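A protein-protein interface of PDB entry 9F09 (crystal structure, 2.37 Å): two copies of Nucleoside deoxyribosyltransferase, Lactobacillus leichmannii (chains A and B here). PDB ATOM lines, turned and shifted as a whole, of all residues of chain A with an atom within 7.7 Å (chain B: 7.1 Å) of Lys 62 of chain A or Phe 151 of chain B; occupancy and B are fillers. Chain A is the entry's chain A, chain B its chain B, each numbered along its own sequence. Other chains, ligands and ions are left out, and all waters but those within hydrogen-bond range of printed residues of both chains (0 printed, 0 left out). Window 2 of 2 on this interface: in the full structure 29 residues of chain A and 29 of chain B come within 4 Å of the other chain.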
ATOM      1  N   TYR A  47      22.399   9.853  20.555  1.00  0.00           N
ATOM      2  CA  TYR A  47      22.047   8.843  19.565  1.00  0.00           C
ATOM      3  C   TYR A  47      22.947   8.971  18.336  1.00  0.00           C
ATOM      4  O   TYR A  47      23.088  10.078  17.789  1.00  0.00           O
ATOM      5  CB  TYR A  47      20.592   8.964  19.093  1.00  0.00           C
ATOM      6  CG  TYR A  47      20.076   7.789  18.256  1.00  0.00           C
ATOM      7  CD1 TYR A  47      20.226   6.469  18.682  1.00  0.00           C
ATOM      8  CD2 TYR A  47      19.392   8.007  17.060  1.00  0.00           C
ATOM      9  CE1 TYR A  47      19.722   5.407  17.940  1.00  0.00           C
ATOM     10  CE2 TYR A  47      18.891   6.954  16.305  1.00  0.00           C
ATOM     11  CZ  TYR A  47      19.066   5.651  16.745  1.00  0.00           C
ATOM     12  OH  TYR A  47      18.590   4.606  16.002  1.00  0.00           O
ATOM     13  N   GLU A  57      21.380  18.982  11.309  1.00  0.00           N
ATOM     14  CA  GLU A  57      20.322  18.350  10.551  1.00  0.00           C
ATOM     15  C   GLU A  57      19.470  17.502  11.494  1.00  0.00           C
ATOM     16  O   GLU A  57      18.318  17.273  11.186  1.00  0.00           O
ATOM     17  CB  GLU A  57      20.858  17.578   9.338  1.00  0.00           C
ATOM     18  CG  GLU A  57      21.773  16.389   9.621  1.00  0.00           C
ATOM     19  CD  GLU A  57      23.269  16.682   9.651  1.00  0.00           C
ATOM     20  OE1 GLU A  57      23.641  17.870   9.857  1.00  0.00           O
ATOM     21  OE2 GLU A  57      24.057  15.725   9.467  1.00  0.00           O
ATOM     22  N   TYR A  58      20.007  17.089  12.653  1.00  0.00           N
ATOM     23  CA  TYR A  58      19.258  16.246  13.578  1.00  0.00           C
ATOM     24  C   TYR A  58      18.435  17.036  14.598  1.00  0.00           C
ATOM     25  O   TYR A  58      17.881  16.444  15.509  1.00  0.00           O
ATOM     26  CB  TYR A  58      20.197  15.313  14.318  1.00  0.00           C
ATOM     27  CG  TYR A  58      20.859  14.232  13.482  1.00  0.00           C
ATOM     28  CD1 TYR A  58      22.078  14.452  12.855  1.00  0.00           C
ATOM     29  CD2 TYR A  58      20.286  12.973  13.369  1.00  0.00           C
ATOM     30  CE1 TYR A  58      22.708  13.445  12.138  1.00  0.00           C
ATOM     31  CE2 TYR A  58      20.897  11.960  12.649  1.00  0.00           C
ATOM     32  CZ  TYR A  58      22.108  12.202  12.021  1.00  0.00           C
ATOM     33  OH  TYR A  58      22.733  11.207  11.320  1.00  0.00           O
ATOM     34  N   LEU A  59      18.249  18.334  14.365  1.00  0.00           N
ATOM     35  CA  LEU A  59      17.582  19.272  15.267  1.00  0.00           C
ATOM     36  C   LEU A  59      16.057  19.208  15.109  1.00  0.00           C
ATOM     37  O   LEU A  59      15.303  19.961  15.760  1.00  0.00           O
ATOM     38  CB  LEU A  59      18.173  20.627  14.833  1.00  0.00           C
ATOM     39  CG  LEU A  59      17.724  21.944  15.494  1.00  0.00           C
ATOM     40  CD1 LEU A  59      18.247  22.180  16.904  1.00  0.00           C
ATOM     41  CD2 LEU A  59      18.168  23.115  14.623  1.00  0.00           C
ATOM     42  N   HIS A  60      15.625  18.392  14.137  1.00  0.00           N
ATOM     43  CA  HIS A  60      14.218  18.200  13.834  1.00  0.00           C
ATOM     44  C   HIS A  60      13.934  16.703  13.680  1.00  0.00           C
ATOM     45  O   HIS A  60      12.760  16.369  13.568  1.00  0.00           O
ATOM     46  CB  HIS A  60      13.775  19.043  12.618  1.00  0.00           C
ATOM     47  CG  HIS A  60      13.477  20.508  12.871  1.00  0.00           C
ATOM     48  ND1 HIS A  60      14.389  21.521  12.614  1.00  0.00           N
ATOM     49  CD2 HIS A  60      12.364  21.138  13.319  1.00  0.00           C
ATOM     50  CE1 HIS A  60      13.848  22.713  12.903  1.00  0.00           C
ATOM     51  NE2 HIS A  60      12.619  22.505  13.333  1.00  0.00           N
ATOM     52  N   ASP A  61      14.970  15.828  13.689  1.00  0.00           N
ATOM     53  CA  ASP A  61      14.796  14.379  13.743  1.00  0.00           C
ATOM     54  C   ASP A  61      14.249  13.947  15.122  1.00  0.00           C
ATOM     55  O   ASP A  61      14.890  14.126  16.159  1.00  0.00           O
ATOM     56  CB  ASP A  61      16.082  13.655  13.359  1.00  0.00           C
ATOM     57  CG  ASP A  61      16.024  12.135  13.346  1.00  0.00           C
ATOM     58  OD1 ASP A  61      14.946  11.612  13.647  1.00  0.00           O
ATOM     59  OD2 ASP A  61      17.049  11.469  13.037  1.00  0.00           O
ATOM     60  N   LYS A  62      13.032  13.391  15.123  1.00  0.00           N
ATOM     61  CA  LYS A  62      12.326  13.001  16.333  1.00  0.00           C
ATOM     62  C   LYS A  62      12.837  11.651  16.831  1.00  0.00           C
ATOM     63  O   LYS A  62      12.686  11.324  17.992  1.00  0.00           O
ATOM     64  CB  LYS A  62      10.817  12.902  16.082  1.00  0.00           C
ATOM     65  CG  LYS A  62      10.130  14.247  15.850  1.00  0.00           C
ATOM     66  CD  LYS A  62       8.677  14.039  15.447  1.00  0.00           C
ATOM     67  CE  LYS A  62       7.799  15.241  15.494  1.00  0.00           C
ATOM     68  NZ  LYS A  62       8.049  16.184  14.401  1.00  0.00           N
ATOM     69  N   VAL A  63      13.426  10.856  15.945  1.00  0.00           N
ATOM     70  CA  VAL A  63      14.036   9.597  16.328  1.00  0.00           C
ATOM     71  C   VAL A  63      15.294   9.881  17.150  1.00  0.00           C
ATOM     72  O   VAL A  63      15.474   9.322  18.230  1.00  0.00           O
ATOM     73  CB  VAL A  63      14.338   8.774  15.061  1.00  0.00           C
ATOM     74  CG1 VAL A  63      15.138   7.498  15.329  1.00  0.00           C
ATOM     75  CG2 VAL A  63      13.062   8.432  14.289  1.00  0.00           C
ATOM     76  N   TRP A  64      16.170  10.747  16.629  1.00  0.00           N
ATOM     77  CA  TRP A  64      17.358  11.138  17.363  1.00  0.00           C
ATOM     78  C   TRP A  64      16.967  11.648  18.750  1.00  0.00           C
ATOM     79  O   TRP A  64      17.575  11.228  19.721  1.00  0.00           O
ATOM     80  CB  TRP A  64      18.199  12.183  16.605  1.00  0.00           C
ATOM     81  CG  TRP A  64      19.356  12.675  17.432  1.00  0.00           C
ATOM     82  CD1 TRP A  64      20.581  12.089  17.579  1.00  0.00           C
ATOM     83  CD2 TRP A  64      19.330  13.804  18.327  1.00  0.00           C
ATOM     84  NE1 TRP A  64      21.334  12.805  18.480  1.00  0.00           N
ATOM     85  CE2 TRP A  64      20.590  13.854  18.958  1.00  0.00           C
ATOM     86  CE3 TRP A  64      18.373  14.767  18.654  1.00  0.00           C
ATOM     87  CZ2 TRP A  64      20.907  14.839  19.886  1.00  0.00           C
ATOM     88  CZ3 TRP A  64      18.675  15.730  19.590  1.00  0.00           C
ATOM     89  CH2 TRP A  64      19.936  15.775  20.184  1.00  0.00           C
ATOM     90  N   ALA A  65      15.962  12.530  18.822  1.00  0.00           N
ATOM     91  CA  ALA A  65      15.526  13.136  20.063  1.00  0.00           C
ATOM     92  C   ALA A  65      14.966  12.087  21.023  1.00  0.00           C
ATOM     93  O   ALA A  65      15.284  12.114  22.208  1.00  0.00           O
ATOM     94  CB  ALA A  65      14.495  14.223  19.788  1.00  0.00           C
ATOM     95  N   THR A  66      14.113  11.188  20.514  1.00  0.00           N
ATOM     96  CA  THR A  66      13.508  10.146  21.327  1.00  0.00           C
ATOM     97  C   THR A  66      14.603   9.302  21.965  1.00  0.00           C
ATOM     98  O   THR A  66      14.599   9.101  23.169  1.00  0.00           O
ATOM     99  CB  THR A  66      12.560   9.270  20.511  1.00  0.00           C
ATOM    100  OG1 THR A  66      11.467  10.083  20.118  1.00  0.00           O
ATOM    101  CG2 THR A  66      11.936   8.172  21.352  1.00  0.00           C
ATOM    102  N   ALA A  67      15.543   8.833  21.139  1.00  0.00           N
ATOM    103  CA  ALA A  67      16.586   7.929  21.591  1.00  0.00           C
ATOM    104  C   ALA A  67      17.536   8.620  22.555  1.00  0.00           C
ATOM    105  O   ALA A  67      17.953   8.010  23.528  1.00  0.00           O
ATOM    106  CB  ALA A  67      17.350   7.359  20.429  1.00  0.00           C
ATOM    107  N   THR A  68      17.858   9.885  22.294  1.00  0.00           N
ATOM    108  CA  THR A  68      18.797  10.593  23.141  1.00  0.00           C
ATOM    109  C   THR A  68      18.130  10.898  24.493  1.00  0.00           C
ATOM    110  O   THR A  68      18.723  10.683  25.541  1.00  0.00           O
ATOM    111  CB  THR A  68      19.305  11.856  22.448  1.00  0.00           C
ATOM    112  OG1 THR A  68      19.968  11.418  21.265  1.00  0.00           O
ATOM    113  CG2 THR A  68      20.343  12.589  23.269  1.00  0.00           C
ATOM    114  N   ASN A  70      15.730   9.243  25.901  1.00  0.00           N
ATOM    115  CA  ASN A  70      15.550   7.991  26.623  1.00  0.00           C
ATOM    116  C   ASN A  70      16.873   7.455  27.166  1.00  0.00           C
ATOM    117  O   ASN A  70      16.923   6.893  28.259  1.00  0.00           O
ATOM    118  CB  ASN A  70      14.750   7.013  25.774  1.00  0.00           C
ATOM    119  CG  ASN A  70      13.279   7.365  25.862  1.00  0.00           C
ATOM    120  OD1 ASN A  70      12.696   7.363  26.950  1.00  0.00           O
ATOM    121  ND2 ASN A  70      12.653   7.742  24.770  1.00  0.00           N
ATOM    122  N   TYR B 118       6.679  30.200  19.242  1.00  0.00           N
ATOM    123  CA  TYR B 118       6.420  28.797  18.964  1.00  0.00           C
ATOM    124  C   TYR B 118       7.217  28.402  17.724  1.00  0.00           C
ATOM    125  O   TYR B 118       7.100  29.041  16.692  1.00  0.00           O
ATOM    126  CB  TYR B 118       4.935  28.474  18.777  1.00  0.00           C
ATOM    127  CG  TYR B 118       4.611  26.984  18.814  1.00  0.00           C
ATOM    128  CD1 TYR B 118       4.686  26.195  17.671  1.00  0.00           C
ATOM    129  CD2 TYR B 118       4.188  26.367  19.992  1.00  0.00           C
ATOM    130  CE1 TYR B 118       4.367  24.841  17.702  1.00  0.00           C
ATOM    131  CE2 TYR B 118       3.891  25.011  20.037  1.00  0.00           C
ATOM    132  CZ  TYR B 118       3.991  24.238  18.890  1.00  0.00           C
ATOM    133  OH  TYR B 118       3.693  22.888  18.949  1.00  0.00           O
ATOM    134  N   TRP B 127      11.536  18.992  25.778  1.00  0.00           N
ATOM    135  CA  TRP B 127      10.838  18.327  24.704  1.00  0.00           C
ATOM    136  C   TRP B 127      10.352  16.952  25.158  1.00  0.00           C
ATOM    137  O   TRP B 127       9.218  16.561  24.890  1.00  0.00           O
ATOM    138  CB  TRP B 127      11.808  18.253  23.516  1.00  0.00           C
ATOM    139  CG  TRP B 127      11.296  17.439  22.362  1.00  0.00           C
ATOM    140  CD1 TRP B 127      10.580  17.892  21.297  1.00  0.00           C
ATOM    141  CD2 TRP B 127      11.474  16.024  22.161  1.00  0.00           C
ATOM    142  NE1 TRP B 127      10.294  16.859  20.451  1.00  0.00           N
ATOM    143  CE2 TRP B 127      10.826  15.703  20.957  1.00  0.00           C
ATOM    144  CE3 TRP B 127      12.095  15.004  22.879  1.00  0.00           C
ATOM    145  CZ2 TRP B 127      10.787  14.403  20.467  1.00  0.00           C
ATOM    146  CZ3 TRP B 127      12.063  13.721  22.390  1.00  0.00           C
ATOM    147  CH2 TRP B 127      11.414  13.425  21.197  1.00  0.00           C
ATOM    148  N   SER B 130       7.701  16.681  28.317  1.00  0.00           N
ATOM    149  CA  SER B 130       6.391  17.198  27.996  1.00  0.00           C
ATOM    150  C   SER B 130       5.579  16.062  27.380  1.00  0.00           C
ATOM    151  O   SER B 130       6.107  15.239  26.638  1.00  0.00           O
ATOM    152  CB  SER B 130       6.504  18.387  27.085  1.00  0.00           C
ATOM    153  OG  SER B 130       6.907  17.950  25.789  1.00  0.00           O
ATOM    154  N   ASP B 131       4.289  16.028  27.707  1.00  0.00           N
ATOM    155  CA  ASP B 131       3.363  15.189  26.966  1.00  0.00           C
ATOM    156  C   ASP B 131       2.838  15.905  25.717  1.00  0.00           C
ATOM    157  O   ASP B 131       2.420  15.271  24.752  1.00  0.00           O
ATOM    158  CB  ASP B 131       2.241  14.746  27.875  1.00  0.00           C
ATOM    159  CG  ASP B 131       2.676  13.807  28.981  1.00  0.00           C
ATOM    160  OD1 ASP B 131       3.256  12.764  28.645  1.00  0.00           O
ATOM    161  OD2 ASP B 131       2.414  14.141  30.168  1.00  0.00           O
ATOM    162  N   ASN B 132       2.919  17.233  25.706  1.00  0.00           N
ATOM    163  CA  ASN B 132       2.446  18.002  24.575  1.00  0.00           C
ATOM    164  C   ASN B 132       2.968  19.424  24.725  1.00  0.00           C
ATOM    165  O   ASN B 132       3.207  19.883  25.848  1.00  0.00           O
ATOM    166  CB  ASN B 132       0.921  17.929  24.533  1.00  0.00           C
ATOM    167  CG  ASN B 132       0.285  18.472  23.276  1.00  0.00           C
ATOM    168  OD1 ASN B 132      -0.942  18.641  23.243  1.00  0.00           O
ATOM    169  ND2 ASN B 132       1.050  18.691  22.220  1.00  0.00           N
ATOM    170  N   VAL B 133       3.130  20.125  23.599  1.00  0.00           N
ATOM    171  CA  VAL B 133       3.440  21.541  23.669  1.00  0.00           C
ATOM    172  C   VAL B 133       2.656  22.313  22.611  1.00  0.00           C
ATOM    173  O   VAL B 133       2.659  21.980  21.434  1.00  0.00           O
ATOM    174  CB  VAL B 133       4.964  21.813  23.693  1.00  0.00           C
ATOM    175  CG1 VAL B 133       5.802  20.574  23.441  1.00  0.00           C
ATOM    176  CG2 VAL B 133       5.418  23.004  22.860  1.00  0.00           C
ATOM    177  N   PHE B 149      -0.997  12.922  23.883  1.00  0.00           N
ATOM    178  CA  PHE B 149       0.418  13.024  23.590  1.00  0.00           C
ATOM    179  C   PHE B 149       0.622  13.611  22.195  1.00  0.00           C
ATOM    180  O   PHE B 149       0.073  13.081  21.244  1.00  0.00           O
ATOM    181  CB  PHE B 149       1.085  11.636  23.595  1.00  0.00           C
ATOM    182  CG  PHE B 149       2.567  11.782  23.300  1.00  0.00           C
ATOM    183  CD1 PHE B 149       3.467  12.093  24.316  1.00  0.00           C
ATOM    184  CD2 PHE B 149       3.040  11.716  21.990  1.00  0.00           C
ATOM    185  CE1 PHE B 149       4.809  12.297  24.023  1.00  0.00           C
ATOM    186  CE2 PHE B 149       4.380  11.896  21.703  1.00  0.00           C
ATOM    187  CZ  PHE B 149       5.262  12.185  22.724  1.00  0.00           C
ATOM    188  N   ASP B 150       1.483  14.625  22.054  1.00  0.00           N
ATOM    189  CA  ASP B 150       1.931  15.024  20.729  1.00  0.00           C
ATOM    190  C   ASP B 150       3.337  15.615  20.804  1.00  0.00           C
ATOM    191  O   ASP B 150       3.798  15.957  21.885  1.00  0.00           O
ATOM    192  CB  ASP B 150       0.960  16.016  20.113  1.00  0.00           C
ATOM    193  CG  ASP B 150       0.914  16.072  18.592  1.00  0.00           C
ATOM    194  OD1 ASP B 150       1.741  15.384  17.935  1.00  0.00           O
ATOM    195  OD2 ASP B 150       0.038  16.811  18.080  1.00  0.00           O
ATOM    196  N   PHE B 151       3.987  15.783  19.643  1.00  0.00           N
ATOM    197  CA  PHE B 151       5.324  16.341  19.591  1.00  0.00           C
ATOM    198  C   PHE B 151       5.260  17.838  19.296  1.00  0.00           C
ATOM    199  O   PHE B 151       4.420  18.281  18.520  1.00  0.00           O
ATOM    200  CB  PHE B 151       6.173  15.684  18.504  1.00  0.00           C
ATOM    201  CG  PHE B 151       6.479  14.202  18.648  1.00  0.00           C
ATOM    202  CD1 PHE B 151       7.409  13.746  19.576  1.00  0.00           C
ATOM    203  CD2 PHE B 151       5.888  13.265  17.805  1.00  0.00           C
ATOM    204  CE1 PHE B 151       7.703  12.393  19.688  1.00  0.00           C
ATOM    205  CE2 PHE B 151       6.174  11.910  17.934  1.00  0.00           C
ATOM    206  CZ  PHE B 151       7.088  11.479  18.868  1.00  0.00           C
ATOM    207  N   TYR B 152       6.171  18.605  19.902  1.00  0.00           N
ATOM    208  CA  TYR B 152       6.442  19.986  19.520  1.00  0.00           C
ATOM    209  C   TYR B 152       6.716  20.076  18.022  1.00  0.00           C
ATOM    210  O   TYR B 152       7.484  19.288  17.482  1.00  0.00           O
ATOM    211  CB  TYR B 152       7.660  20.494  20.292  1.00  0.00           C
ATOM    212  CG  TYR B 152       8.068  21.955  20.152  1.00  0.00           C
ATOM    213  CD1 TYR B 152       7.137  22.986  20.086  1.00  0.00           C
ATOM    214  CD2 TYR B 152       9.408  22.308  20.130  1.00  0.00           C
ATOM    215  CE1 TYR B 152       7.531  24.316  20.000  1.00  0.00           C
ATOM    216  CE2 TYR B 152       9.814  23.628  20.066  1.00  0.00           C
ATOM    217  CZ  TYR B 152       8.878  24.636  19.968  1.00  0.00           C
ATOM    218  OH  TYR B 152       9.361  25.908  19.884  1.00  0.00           O
ATOM    219  N   GLU B 153       6.040  21.027  17.369  1.00  0.00           N
ATOM    220  CA  GLU B 153       6.271  21.355  15.969  1.00  0.00           C
ATOM    221  C   GLU B 153       7.293  22.491  15.981  1.00  0.00           C
ATOM    222  O   GLU B 153       6.938  23.662  15.856  1.00  0.00           O
ATOM    223  CB  GLU B 153       4.944  21.653  15.250  1.00  0.00           C
ATOM    224  N   GLY B 154       8.558  22.120  16.220  1.00  0.00           N
ATOM    225  CA  GLY B 154       9.612  23.086  16.448  1.00  0.00           C
ATOM    226  C   GLY B 154      10.942  22.409  16.717  1.00  0.00           C
ATOM    227  O   GLY B 154      11.031  21.199  16.724  1.00  0.00           O
ATOM    228  N   VAL B 156      14.628  21.419  18.630  1.00  0.00           N
ATOM    229  CA  VAL B 156      15.112  21.014  19.942  1.00  0.00           C
ATOM    230  C   VAL B 156      16.627  20.832  19.879  1.00  0.00           C
ATOM    231  O   VAL B 156      17.109  20.120  19.000  1.00  0.00           O
ATOM    232  CB  VAL B 156      14.349  19.771  20.451  1.00  0.00           C
ATOM    233  CG1 VAL B 156      13.497  19.093  19.383  1.00  0.00           C
ATOM    234  CG2 VAL B 156      15.264  18.754  21.107  1.00  0.00           C
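O of Leu 59 of chain A is in hydrogen-bond range of N of Val 156 of chain B (3.3 Å).
Among the printed residues, pairs that only touch across the chains: His 60 of chain A with Gly 154 of chain B, Lys 62 of chain A with Phe 151 of chain B, Ala 65 of chain A with Trp 127 of chain B and Thr 66 of chain A with Trp 127 of chain B.
O of Thr 66 of chain A sits at hydrogen-bond distance from ND2 of Asn 70 of chain A (2.9 Å).
The backbone carbonyl oxygen of Lys 62 of chain A is in hydrogen-bond range of the side-chain hydroxyl of Thr 66 of chain A, at 2.7 Å.
The side-chain hydroxyl of Ser 130 of chain B lies within hydrogen-bond range of the backbone carbonyl oxygen of Trp 127 of chain B (2.8 Å).
Of chain B, only Phe 151 (3.4 Å) comes within 4 Å of Lys 62 of chain A.
Of the printed residues of chain A, Phe 151 of chain B touches Lys 62.
Printed residues of chain A within 4 Å of Gly 154 of chain B: His 60.
Printed residues of chain B within 4 Å of His 60 of chain A: Gly 154 (3.7 Å).
Of the printed residues of chain B, Ala 65 of chain A touches Trp 127.
Ala 67 of chain A touches none of the printed residues of chain B.
The nearest residue of chain B that does not touch Lys 62 of chain A is Trp 127 of chain B (4.04 Å).
The nearest printed residue of chain A that does not touch Val 156 of chain B is Trp 64 of chain A (4.7 Å).
Hydrophobic or aromatic side chains of chain B within 4 Å of the printed part of chain A: Trp 127 and Phe 151.
Of the 14 printed residues of chain A, 5 touch a printed residue of chain B.
Hydrophobic or aromatic side chains of chain A within 4 Å of the printed part of chain B: Leu 59, His 60 and Ala 65.
Among the printed residues, 5 pairs touch across the chains.
Among the printed residues, no Asp or Glu carboxylate lies within 4 Å of a Lys or Arg side-chain nitrogen of the other chain.
No position is printed for both chains.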
